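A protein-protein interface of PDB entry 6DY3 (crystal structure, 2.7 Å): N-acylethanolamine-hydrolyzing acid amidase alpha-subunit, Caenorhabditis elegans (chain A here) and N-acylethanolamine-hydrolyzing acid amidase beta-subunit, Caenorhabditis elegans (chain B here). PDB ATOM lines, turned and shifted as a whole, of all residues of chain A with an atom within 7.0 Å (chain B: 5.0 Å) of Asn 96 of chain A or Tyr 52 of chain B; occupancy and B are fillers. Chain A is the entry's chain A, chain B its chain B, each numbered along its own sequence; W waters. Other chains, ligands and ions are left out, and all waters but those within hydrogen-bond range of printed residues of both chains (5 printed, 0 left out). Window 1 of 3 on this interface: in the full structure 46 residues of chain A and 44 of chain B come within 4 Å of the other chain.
Printed residues of chain B within 4 Å of Asn 96 of chain A: Leu 51 (3.0 Å), Tyr 52 (3.4 Å), Asn 53 (3.3 Å), Ser 93 (3.99 Å) and Phe 94 (3.5 Å). Of the printed residues of chain A, Tyr 52 of chain B touches Met 95 (3.4 Å) and Asn 96 (3.4 Å). Of the printed residues of chain B, Ile 81 of chain A touches Leu 51 and Asn 53. Of the printed residues of chain A, Leu 51 of chain B touches Ile 33 (3.9 Å), Ile 81 (3.7 Å) and Asn 96 (3.0 Å). Of the printed residues of chain B, Ile 33 of chain A touches Leu 51. Of the printed residues of chain A, Phe 94 of chain B touches Phe 70 (3.5 Å) and Asn 96 (3.5 Å). Glu 91 of chain A touches none of the printed residues of chain B. Phe 49 of chain B touches none of the printed residues of chain A. The nearest printed residue of chain B that does not touch Asn 96 of chain A is Gly 54 of chain B (4.2 Å). The nearest residue of chain A that does not touch Tyr 52 of chain B is Thr 47 of chain A (4.1 Å). The nearest printed residue of chain B that does not touch Met 95 of chain A is Leu 51 of chain B (4.7 Å).
The backbone carbonyl oxygen of Ile 92 of chain A sits at hydrogen-bond distance from the side-chain amide nitrogen of Asn 96 of chain A. The side-chain hydroxyl (OG1) of Thr 48 of chain B lies within hydrogen-bond range of the backbone carbonyl oxygen (O) of Tyr 52 of chain B.
Among the printed residues, pairs that only touch across the chains: Trp 29 of chain A with Asn 53 of chain B (3.4 Å), Ile 33 of chain A with Leu 51 of chain B (3.9 Å), Phe 70 of chain A with Phe 94 of chain B (3.5 Å), Leu 78 of chain A with Asn 53 of chain B (3.3 Å), Ile 81 of chain A with Leu 51 of chain B (3.7 Å), Ile 81 of chain A with Asn 53 of chain B (3.98 Å), Met 95 of chain A with Tyr 52 of chain B (3.4 Å), Asn 96 of chain A with Tyr 52 of chain B (3.4 Å), Asn 96 of chain A with Ser 93 of chain B (3.99 Å), Asn 96 of chain A with Phe 94 of chain B (3.5 Å) and Ala 102 of chain A with Tyr 21 of chain B (3.3 Å).
The side-chain amide nitrogen of Asn 96 of chain A lies within hydrogen-bond range of the backbone carbonyl oxygen of Leu 51 of chain B (3.0 Å). The side-chain amide oxygen of Asn 96 of chain A lies close to the side-chain amide oxygen of Asn 53 of chain B, 3.3 Å away.
Of the 10 printed residues of chain B, 6 touch a printed residue of chain A. Hydrophobic or aromatic side chains of chain B that line the printed part of chain A: Tyr 21, Leu 51, Tyr 52 and Phe 94. Printed residues of chain A that touch a printed residue of chain B: Trp 29, Ile 33, Phe 70, Leu 78, Ile 81, Met 95, Asn 96 and Ala 102. Hydrophobic or aromatic side chains of chain A that line the printed part of chain B: Trp 29, Ile 33, Phe 70, Leu 78, Ile 81, Met 95 and Ala 102. Among the printed residues, 13 pairs touch across the chains. Among the printed residues, no Asp or Glu carboxylate lies within 4 Å of a Lys or Arg side-chain nitrogen of the other chain.
Water W2 lies within hydrogen-bond range of OH of Tyr 21 of chain B (2.5 Å), O of Tyr 99 of chain A (2.7 Å), N of Ala 102 of chain A (3.0 Å) and N of Val 101 of chain A (3.1 Å). Water W1 lies within hydrogen-bond range of the side-chain amide oxygen of Asn 96 of chain A (2.6 Å), the backbone NH of Gly 54 of chain B (3.0 Å) and the side-chain hydroxyl of Ser 93 of chain B (3.0 Å). Water W3 bridges O of Asn 96 of chain A (2.6 Å) and N of Ser 93 of chain B (2.8 Å). Water W4 lies within hydrogen-bond range of OH of Tyr 52 of chain B (2.6 Å), O of Met 95 of chain A (3.2 Å) and O of Leu 98 of chain A (3.3 Å). Water W5 lies within hydrogen-bond range of OH of Tyr 52 of chain B (2.7 Å), OH of Tyr 21 of chain B (2.7 Å) and OG1 of Thr 47 of chain A (3.1 Å).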
ATOM      1  N   TRP A  29      40.840 -26.911 -15.832  1.00  0.00           N
ATOM      2  CA  TRP A  29      40.221 -27.147 -17.126  1.00  0.00           C
ATOM      3  C   TRP A  29      40.733 -26.198 -18.201  1.00  0.00           C
ATOM      4  O   TRP A  29      40.146 -26.138 -19.286  1.00  0.00           O
ATOM      5  CB  TRP A  29      38.702 -27.025 -17.002  1.00  0.00           C
ATOM      6  CG  TRP A  29      38.113 -28.023 -16.062  1.00  0.00           C
ATOM      7  CD1 TRP A  29      37.771 -27.821 -14.754  1.00  0.00           C
ATOM      8  CD2 TRP A  29      37.807 -29.391 -16.352  1.00  0.00           C
ATOM      9  NE1 TRP A  29      37.266 -28.981 -14.215  1.00  0.00           N
ATOM     10  CE2 TRP A  29      37.280 -29.958 -15.176  1.00  0.00           C
ATOM     11  CE3 TRP A  29      37.925 -30.190 -17.494  1.00  0.00           C
ATOM     12  CZ2 TRP A  29      36.872 -31.285 -15.111  1.00  0.00           C
ATOM     13  CZ3 TRP A  29      37.518 -31.507 -17.426  1.00  0.00           C
ATOM     14  CH2 TRP A  29      36.999 -32.042 -16.247  1.00  0.00           C
ATOM     15  N   VAL A  32      41.576 -27.979 -21.582  1.00  0.00           N
ATOM     16  CA  VAL A  32      40.356 -28.490 -22.202  1.00  0.00           C
ATOM     17  C   VAL A  32      39.593 -27.356 -22.875  1.00  0.00           C
ATOM     18  O   VAL A  32      39.174 -27.466 -24.034  1.00  0.00           O
ATOM     19  CB  VAL A  32      39.488 -29.215 -21.156  1.00  0.00           C
ATOM     20  CG1 VAL A  32      38.104 -29.543 -21.718  1.00  0.00           C
ATOM     21  CG2 VAL A  32      40.184 -30.485 -20.680  1.00  0.00           C
ATOM     22  N   ILE A  33      39.389 -26.249 -22.153  1.00  0.00           N
ATOM     23  CA  ILE A  33      38.647 -25.121 -22.711  1.00  0.00           C
ATOM     24  C   ILE A  33      39.403 -24.521 -23.890  1.00  0.00           C
ATOM     25  O   ILE A  33      38.812 -24.199 -24.929  1.00  0.00           O
ATOM     26  CB  ILE A  33      38.375 -24.069 -21.617  1.00  0.00           C
ATOM     27  CG1 ILE A  33      37.515 -24.654 -20.488  1.00  0.00           C
ATOM     28  CG2 ILE A  33      37.710 -22.829 -22.205  1.00  0.00           C
ATOM     29  CD1 ILE A  33      36.173 -25.204 -20.932  1.00  0.00           C
ATOM     30  N   VAL A  43      27.685 -24.222 -28.566  1.00  0.00           N
ATOM     31  CA  VAL A  43      27.087 -25.233 -27.697  1.00  0.00           C
ATOM     32  C   VAL A  43      26.195 -24.571 -26.661  1.00  0.00           C
ATOM     33  O   VAL A  43      25.059 -25.000 -26.424  1.00  0.00           O
ATOM     34  CB  VAL A  43      28.184 -26.087 -27.035  1.00  0.00           C
ATOM     35  CG1 VAL A  43      27.639 -26.848 -25.829  1.00  0.00           C
ATOM     36  CG2 VAL A  43      28.771 -27.062 -28.053  1.00  0.00           C
ATOM     37  N   THR A  47      22.275 -25.128 -26.379  1.00  0.00           N
ATOM     38  CA  THR A  47      21.756 -25.830 -25.208  1.00  0.00           C
ATOM     39  C   THR A  47      20.641 -25.040 -24.532  1.00  0.00           C
ATOM     40  O   THR A  47      19.640 -25.622 -24.097  1.00  0.00           O
ATOM     41  CB  THR A  47      22.884 -26.108 -24.213  1.00  0.00           C
ATOM     42  OG1 THR A  47      23.922 -26.841 -24.865  1.00  0.00           O
ATOM     43  CG2 THR A  47      22.379 -26.924 -23.033  1.00  0.00           C
ATOM     44  N   PHE A  70      27.196 -25.929  -4.737  1.00  0.00           N
ATOM     45  CA  PHE A  70      28.459 -26.613  -4.952  1.00  0.00           C
ATOM     46  C   PHE A  70      29.410 -26.354  -3.792  1.00  0.00           C
ATOM     47  O   PHE A  70      29.293 -25.363  -3.067  1.00  0.00           O
ATOM     48  CB  PHE A  70      29.129 -26.155  -6.259  1.00  0.00           C
ATOM     49  CG  PHE A  70      28.216 -26.161  -7.450  1.00  0.00           C
ATOM     50  CD1 PHE A  70      27.893 -27.350  -8.098  1.00  0.00           C
ATOM     51  CD2 PHE A  70      27.692 -24.976  -7.936  1.00  0.00           C
ATOM     52  CE1 PHE A  70      27.056 -27.353  -9.202  1.00  0.00           C
ATOM     53  CE2 PHE A  70      26.853 -24.972  -9.041  1.00  0.00           C
ATOM     54  CZ  PHE A  70      26.536 -26.161  -9.675  1.00  0.00           C
ATOM     55  N   LEU A  78      34.129 -24.034 -11.799  1.00  0.00           N
ATOM     56  CA  LEU A  78      33.132 -23.413 -12.663  1.00  0.00           C
ATOM     57  C   LEU A  78      33.508 -21.975 -12.987  1.00  0.00           C
ATOM     58  O   LEU A  78      33.361 -21.531 -14.132  1.00  0.00           O
ATOM     59  CB  LEU A  78      31.761 -23.476 -11.997  1.00  0.00           C
ATOM     60  CG  LEU A  78      31.158 -24.877 -11.881  1.00  0.00           C
ATOM     61  CD1 LEU A  78      29.960 -24.860 -10.942  1.00  0.00           C
ATOM     62  CD2 LEU A  78      30.762 -25.426 -13.260  1.00  0.00           C
ATOM     63  N   ILE A  81      36.274 -22.145 -15.456  1.00  0.00           N
ATOM     64  CA  ILE A  81      35.756 -22.505 -16.773  1.00  0.00           C
ATOM     65  C   ILE A  81      35.128 -21.289 -17.441  1.00  0.00           C
ATOM     66  O   ILE A  81      35.334 -21.044 -18.635  1.00  0.00           O
ATOM     67  CB  ILE A  81      34.755 -23.671 -16.656  1.00  0.00           C
ATOM     68  CG1 ILE A  81      35.497 -24.964 -16.300  1.00  0.00           C
ATOM     69  CG2 ILE A  81      33.965 -23.845 -17.960  1.00  0.00           C
ATOM     70  CD1 ILE A  81      34.585 -26.152 -16.046  1.00  0.00           C
ATOM     71  N   GLU A  91      25.199 -19.176 -17.024  1.00  0.00           N
ATOM     72  CA  GLU A  91      24.800 -20.153 -18.032  1.00  0.00           C
ATOM     73  C   GLU A  91      25.559 -21.461 -17.854  1.00  0.00           C
ATOM     74  O   GLU A  91      24.982 -22.546 -17.985  1.00  0.00           O
ATOM     75  CB  GLU A  91      25.023 -19.576 -19.432  1.00  0.00           C
ATOM     76  CG  GLU A  91      24.140 -18.365 -19.743  1.00  0.00           C
ATOM     77  CD  GLU A  91      24.376 -17.786 -21.133  1.00  0.00           C
ATOM     78  OE1 GLU A  91      25.320 -18.232 -21.819  1.00  0.00           O
ATOM     79  OE2 GLU A  91      23.621 -16.875 -21.537  1.00  0.00           O
ATOM     80  N   ILE A  92      26.847 -21.376 -17.525  1.00  0.00           N
ATOM     81  CA  ILE A  92      27.643 -22.582 -17.315  1.00  0.00           C
ATOM     82  C   ILE A  92      27.124 -23.360 -16.114  1.00  0.00           C
ATOM     83  O   ILE A  92      27.025 -24.593 -16.151  1.00  0.00           O
ATOM     84  CB  ILE A  92      29.130 -22.208 -17.167  1.00  0.00           C
ATOM     85  CG1 ILE A  92      29.679 -21.801 -18.537  1.00  0.00           C
ATOM     86  CG2 ILE A  92      29.938 -23.359 -16.540  1.00  0.00           C
ATOM     87  CD1 ILE A  92      31.071 -21.231 -18.503  1.00  0.00           C
ATOM     88  N   VAL A  93      26.790 -22.656 -15.029  1.00  0.00           N
ATOM     89  CA  VAL A  93      26.215 -23.317 -13.859  1.00  0.00           C
ATOM     90  C   VAL A  93      24.887 -23.975 -14.221  1.00  0.00           C
ATOM     91  O   VAL A  93      24.613 -25.115 -13.826  1.00  0.00           O
ATOM     92  CB  VAL A  93      26.047 -22.305 -12.707  1.00  0.00           C
ATOM     93  CG1 VAL A  93      25.213 -22.906 -11.564  1.00  0.00           C
ATOM     94  CG2 VAL A  93      27.407 -21.847 -12.199  1.00  0.00           C
ATOM     95  N   GLY A  94      24.038 -23.263 -14.968  1.00  0.00           N
ATOM     96  CA  GLY A  94      22.751 -23.819 -15.341  1.00  0.00           C
ATOM     97  C   GLY A  94      22.869 -25.098 -16.153  1.00  0.00           C
ATOM     98  O   GLY A  94      22.176 -26.082 -15.889  1.00  0.00           O
ATOM     99  N   MET A  95      23.753 -25.106 -17.158  1.00  0.00           N
ATOM    100  CA  MET A  95      23.904 -26.313 -17.967  1.00  0.00           C
ATOM    101  C   MET A  95      24.413 -27.484 -17.143  1.00  0.00           C
ATOM    102  O   MET A  95      23.995 -28.630 -17.364  1.00  0.00           O
ATOM    103  CB  MET A  95      24.822 -26.065 -19.159  1.00  0.00           C
ATOM    104  CG  MET A  95      24.156 -25.290 -20.276  1.00  0.00           C
ATOM    105  SD  MET A  95      25.244 -24.967 -21.663  1.00  0.00           S
ATOM    106  CE  MET A  95      26.133 -23.572 -21.007  1.00  0.00           C
ATOM    107  N   ASN A  96      25.314 -27.237 -16.200  1.00  0.00           N
ATOM    108  CA  ASN A  96      25.846 -28.336 -15.398  1.00  0.00           C
ATOM    109  C   ASN A  96      24.794 -28.916 -14.465  1.00  0.00           C
ATOM    110  O   ASN A  96      24.801 -30.119 -14.193  1.00  0.00           O
ATOM    111  CB  ASN A  96      27.051 -27.836 -14.613  1.00  0.00           C
ATOM    112  CG  ASN A  96      28.330 -27.925 -15.393  1.00  0.00           C
ATOM    113  OD1 ASN A  96      29.006 -28.953 -15.367  1.00  0.00           O
ATOM    114  ND2 ASN A  96      28.678 -26.850 -16.101  1.00  0.00           N
ATOM    115  N   ILE A  97      23.904 -28.074 -13.948  1.00  0.00           N
ATOM    116  CA  ILE A  97      22.849 -28.552 -13.056  1.00  0.00           C
ATOM    117  C   ILE A  97      21.766 -29.279 -13.847  1.00  0.00           C
ATOM    118  O   ILE A  97      21.336 -30.379 -13.478  1.00  0.00           O
ATOM    119  CB  ILE A  97      22.266 -27.379 -12.241  1.00  0.00           C
ATOM    120  CG1 ILE A  97      23.291 -26.919 -11.195  1.00  0.00           C
ATOM    121  CG2 ILE A  97      20.944 -27.778 -11.579  1.00  0.00           C
ATOM    122  CD1 ILE A  97      22.849 -25.765 -10.337  1.00  0.00           C
ATOM    123  N   LEU A  98      21.311 -28.674 -14.943  1.00  0.00           N
ATOM    124  CA  LEU A  98      20.342 -29.307 -15.841  1.00  0.00           C
ATOM    125  C   LEU A  98      21.093 -30.187 -16.844  1.00  0.00           C
ATOM    126  O   LEU A  98      21.125 -29.939 -18.054  1.00  0.00           O
ATOM    127  CB  LEU A  98      19.498 -28.249 -16.536  1.00  0.00           C
ATOM    128  CG  LEU A  98      18.807 -27.241 -15.609  1.00  0.00           C
ATOM    129  CD1 LEU A  98      17.942 -26.285 -16.405  1.00  0.00           C
ATOM    130  CD2 LEU A  98      17.987 -27.938 -14.535  1.00  0.00           C
ATOM    131  N   TYR A  99      21.690 -31.254 -16.300  1.00  0.00           N
ATOM    132  CA  TYR A  99      22.645 -32.053 -17.061  1.00  0.00           C
ATOM    133  C   TYR A  99      22.012 -32.668 -18.305  1.00  0.00           C
ATOM    134  O   TYR A  99      22.702 -32.864 -19.310  1.00  0.00           O
ATOM    135  CB  TYR A  99      23.245 -33.150 -16.167  1.00  0.00           C
ATOM    136  CG  TYR A  99      22.243 -34.168 -15.660  1.00  0.00           C
ATOM    137  CD1 TYR A  99      22.014 -35.350 -16.357  1.00  0.00           C
ATOM    138  CD2 TYR A  99      21.527 -33.949 -14.492  1.00  0.00           C
ATOM    139  CE1 TYR A  99      21.094 -36.284 -15.906  1.00  0.00           C
ATOM    140  CE2 TYR A  99      20.603 -34.876 -14.032  1.00  0.00           C
ATOM    141  CZ  TYR A  99      20.390 -36.043 -14.743  1.00  0.00           C
ATOM    142  OH  TYR A  99      19.468 -36.971 -14.293  1.00  0.00           O
ATOM    143  N   ASP A 100      20.707 -32.949 -18.275  1.00  0.00           N
ATOM    144  CA  ASP A 100      20.036 -33.667 -19.354  1.00  0.00           C
ATOM    145  C   ASP A 100      19.057 -32.789 -20.128  1.00  0.00           C
ATOM    146  O   ASP A 100      18.206 -33.312 -20.855  1.00  0.00           O
ATOM    147  CB  ASP A 100      19.299 -34.884 -18.796  1.00  0.00           C
ATOM    148  CG  ASP A 100      18.089 -34.492 -17.957  1.00  0.00           C
ATOM    149  OD1 ASP A 100      18.079 -33.360 -17.425  1.00  0.00           O
ATOM    150  OD2 ASP A 100      17.144 -35.303 -17.840  1.00  0.00           O
ATOM    151  N   VAL A 101      19.157 -31.466 -19.999  1.00  0.00           N
ATOM    152  CA  VAL A 101      18.140 -30.610 -20.596  1.00  0.00           C
ATOM    153  C   VAL A 101      18.159 -30.724 -22.114  1.00  0.00           C
ATOM    154  O   VAL A 101      17.108 -30.645 -22.762  1.00  0.00           O
ATOM    155  CB  VAL A 101      18.328 -29.153 -20.134  1.00  0.00           C
ATOM    156  CG1 VAL A 101      19.620 -28.561 -20.691  1.00  0.00           C
ATOM    157  CG2 VAL A 101      17.131 -28.320 -20.525  1.00  0.00           C
ATOM    158  N   ALA A 102      19.335 -30.909 -22.709  1.00  0.00           N
ATOM    159  CA  ALA A 102      19.458 -31.043 -24.153  1.00  0.00           C
ATOM    160  C   ALA A 102      19.574 -32.492 -24.594  1.00  0.00           C
ATOM    161  O   ALA A 102      19.745 -32.752 -25.787  1.00  0.00           O
ATOM    162  CB  ALA A 102      20.663 -30.244 -24.660  1.00  0.00           C
ATOM    163  N   TYR B  21      21.867 -38.225 -27.203  1.00  0.00           N
ATOM    164  CA  TYR B  21      21.745 -36.810 -26.891  1.00  0.00           C
ATOM    165  C   TYR B  21      21.094 -36.127 -28.078  1.00  0.00           C
ATOM    166  O   TYR B  21      21.540 -36.312 -29.214  1.00  0.00           O
ATOM    167  CB  TYR B  21      23.126 -36.211 -26.618  1.00  0.00           C
ATOM    168  CG  TYR B  21      23.164 -34.988 -25.738  1.00  0.00           C
ATOM    169  CD1 TYR B  21      23.117 -35.100 -24.353  1.00  0.00           C
ATOM    170  CD2 TYR B  21      23.295 -33.719 -26.293  1.00  0.00           C
ATOM    171  CE1 TYR B  21      23.176 -33.986 -23.547  1.00  0.00           C
ATOM    172  CE2 TYR B  21      23.356 -32.588 -25.489  1.00  0.00           C
ATOM    173  CZ  TYR B  21      23.297 -32.730 -24.119  1.00  0.00           C
ATOM    174  OH  TYR B  21      23.362 -31.605 -23.326  1.00  0.00           O
ATOM    175  N   THR B  48      33.301 -36.830 -20.305  1.00  0.00           N
ATOM    176  CA  THR B  48      32.536 -35.616 -20.083  1.00  0.00           C
ATOM    177  C   THR B  48      32.673 -34.755 -21.330  1.00  0.00           C
ATOM    178  O   THR B  48      33.159 -35.211 -22.372  1.00  0.00           O
ATOM    179  CB  THR B  48      32.992 -34.892 -18.808  1.00  0.00           C
ATOM    180  OG1 THR B  48      32.112 -33.791 -18.546  1.00  0.00           O
ATOM    181  CG2 THR B  48      34.430 -34.382 -18.942  1.00  0.00           C
ATOM    182  N   PHE B  49      32.267 -33.496 -21.219  1.00  0.00           N
ATOM    183  CA  PHE B  49      32.269 -32.591 -22.354  1.00  0.00           C
ATOM    184  C   PHE B  49      32.810 -31.244 -21.907  1.00  0.00           C
ATOM    185  O   PHE B  49      32.669 -30.859 -20.746  1.00  0.00           O
ATOM    186  CB  PHE B  49      30.859 -32.459 -22.931  1.00  0.00           C
ATOM    187  CG  PHE B  49      30.093 -33.754 -22.934  1.00  0.00           C
ATOM    188  CD1 PHE B  49      29.378 -34.156 -21.815  1.00  0.00           C
ATOM    189  CD2 PHE B  49      30.102 -34.579 -24.046  1.00  0.00           C
ATOM    190  CE1 PHE B  49      28.680 -35.345 -21.806  1.00  0.00           C
ATOM    191  CE2 PHE B  49      29.400 -35.776 -24.044  1.00  0.00           C
ATOM    192  CZ  PHE B  49      28.689 -36.157 -22.921  1.00  0.00           C
ATOM    193  N   ALA B  50      33.448 -30.538 -22.835  1.00  0.00           N
ATOM    194  CA  ALA B  50      33.968 -29.214 -22.524  1.00  0.00           C
ATOM    195  C   ALA B  50      32.861 -28.348 -21.941  1.00  0.00           C
ATOM    196  O   ALA B  50      31.764 -28.277 -22.495  1.00  0.00           O
ATOM    197  CB  ALA B  50      34.544 -28.570 -23.785  1.00  0.00           C
ATOM    198  N   LEU B  51      33.171 -27.692 -20.816  1.00  0.00           N
ATOM    199  CA  LEU B  51      32.248 -26.868 -20.029  1.00  0.00           C
ATOM    200  C   LEU B  51      31.599 -27.650 -18.892  1.00  0.00           C
ATOM    201  O   LEU B  51      31.094 -27.047 -17.939  1.00  0.00           O
ATOM    202  CB  LEU B  51      31.141 -26.234 -20.882  1.00  0.00           C
ATOM    203  CG  LEU B  51      31.577 -25.210 -21.931  1.00  0.00           C
ATOM    204  CD1 LEU B  51      30.372 -24.745 -22.739  1.00  0.00           C
ATOM    205  CD2 LEU B  51      32.282 -24.021 -21.289  1.00  0.00           C
ATOM    206  N   TYR B  52      31.617 -28.976 -18.966  1.00  0.00           N
ATOM    207  CA  TYR B  52      31.034 -29.830 -17.937  1.00  0.00           C
ATOM    208  C   TYR B  52      32.151 -30.489 -17.138  1.00  0.00           C
ATOM    209  O   TYR B  52      32.934 -31.268 -17.691  1.00  0.00           O
ATOM    210  CB  TYR B  52      30.133 -30.893 -18.562  1.00  0.00           C
ATOM    211  CG  TYR B  52      28.931 -30.328 -19.288  1.00  0.00           C
ATOM    212  CD1 TYR B  52      29.019 -29.945 -20.616  1.00  0.00           C
ATOM    213  CD2 TYR B  52      27.713 -30.177 -18.646  1.00  0.00           C
ATOM    214  CE1 TYR B  52      27.935 -29.426 -21.281  1.00  0.00           C
ATOM    215  CE2 TYR B  52      26.625 -29.662 -19.304  1.00  0.00           C
ATOM    216  CZ  TYR B  52      26.738 -29.286 -20.620  1.00  0.00           C
ATOM    217  OH  TYR B  52      25.649 -28.766 -21.286  1.00  0.00           O
ATOM    218  N   ASN B  53      32.221 -30.188 -15.842  1.00  0.00           N
ATOM    219  CA  ASN B  53      33.251 -30.755 -14.978  1.00  0.00           C
ATOM    220  C   ASN B  53      32.700 -31.819 -14.034  1.00  0.00           C
ATOM    221  O   ASN B  53      33.420 -32.281 -13.144  1.00  0.00           O
ATOM    222  CB  ASN B  53      33.969 -29.650 -14.188  1.00  0.00           C
ATOM    223  CG  ASN B  53      33.018 -28.736 -13.451  1.00  0.00           C
ATOM    224  OD1 ASN B  53      31.909 -28.471 -13.911  1.00  0.00           O
ATOM    225  ND2 ASN B  53      33.457 -28.234 -12.300  1.00  0.00           N
ATOM    226  N   GLY B  54      31.441 -32.227 -14.212  1.00  0.00           N
ATOM    227  CA  GLY B  54      30.922 -33.407 -13.558  1.00  0.00           C
ATOM    228  C   GLY B  54      31.180 -34.649 -14.391  1.00  0.00           C
ATOM    229  O   GLY B  54      31.702 -34.586 -15.502  1.00  0.00           O
ATOM    230  N   SER B  93      25.645 -34.603 -11.617  1.00  0.00           N
ATOM    231  CA  SER B  93      26.955 -34.948 -12.168  1.00  0.00           C
ATOM    232  C   SER B  93      28.059 -34.800 -11.128  1.00  0.00           C
ATOM    233  O   SER B  93      29.043 -35.549 -11.155  1.00  0.00           O
ATOM    234  CB  SER B  93      27.270 -34.081 -13.387  1.00  0.00           C
ATOM    235  OG  SER B  93      27.552 -32.747 -13.006  1.00  0.00           O
ATOM    236  N   PHE B  94      27.918 -33.844 -10.208  1.00  0.00           N
ATOM    237  CA  PHE B  94      28.940 -33.645  -9.190  1.00  0.00           C
ATOM    238  C   PHE B  94      28.786 -34.619  -8.035  1.00  0.00           C
ATOM    239  O   PHE B  94      29.776 -34.960  -7.376  1.00  0.00           O
ATOM    240  CB  PHE B  94      28.902 -32.198  -8.707  1.00  0.00           C
ATOM    241  CG  PHE B  94      29.132 -31.217  -9.808  1.00  0.00           C
ATOM    242  CD1 PHE B  94      28.065 -30.643 -10.467  1.00  0.00           C
ATOM    243  CD2 PHE B  94      30.422 -30.913 -10.228  1.00  0.00           C
ATOM    244  CE1 PHE B  94      28.272 -29.758 -11.504  1.00  0.00           C
ATOM    245  CE2 PHE B  94      30.635 -30.024 -11.269  1.00  0.00           C
ATOM    246  CZ  PHE B  94      29.554 -29.448 -11.906  1.00  0.00           C
HETATM  247  O   HOH W   1      28.840 -31.564 -15.502  1.00  0.00           O
HETATM  248  O   HOH W   2      21.917 -31.251 -21.305  1.00  0.00           O
HETATM  249  O   HOH W   3      24.759 -31.998 -12.338  1.00  0.00           O
HETATM  250  O   HOH W   4      23.165 -28.914 -20.391  1.00  0.00           O
HETATM  251  O   HOH W   5      25.046 -29.547 -23.793  1.00  0.00           O
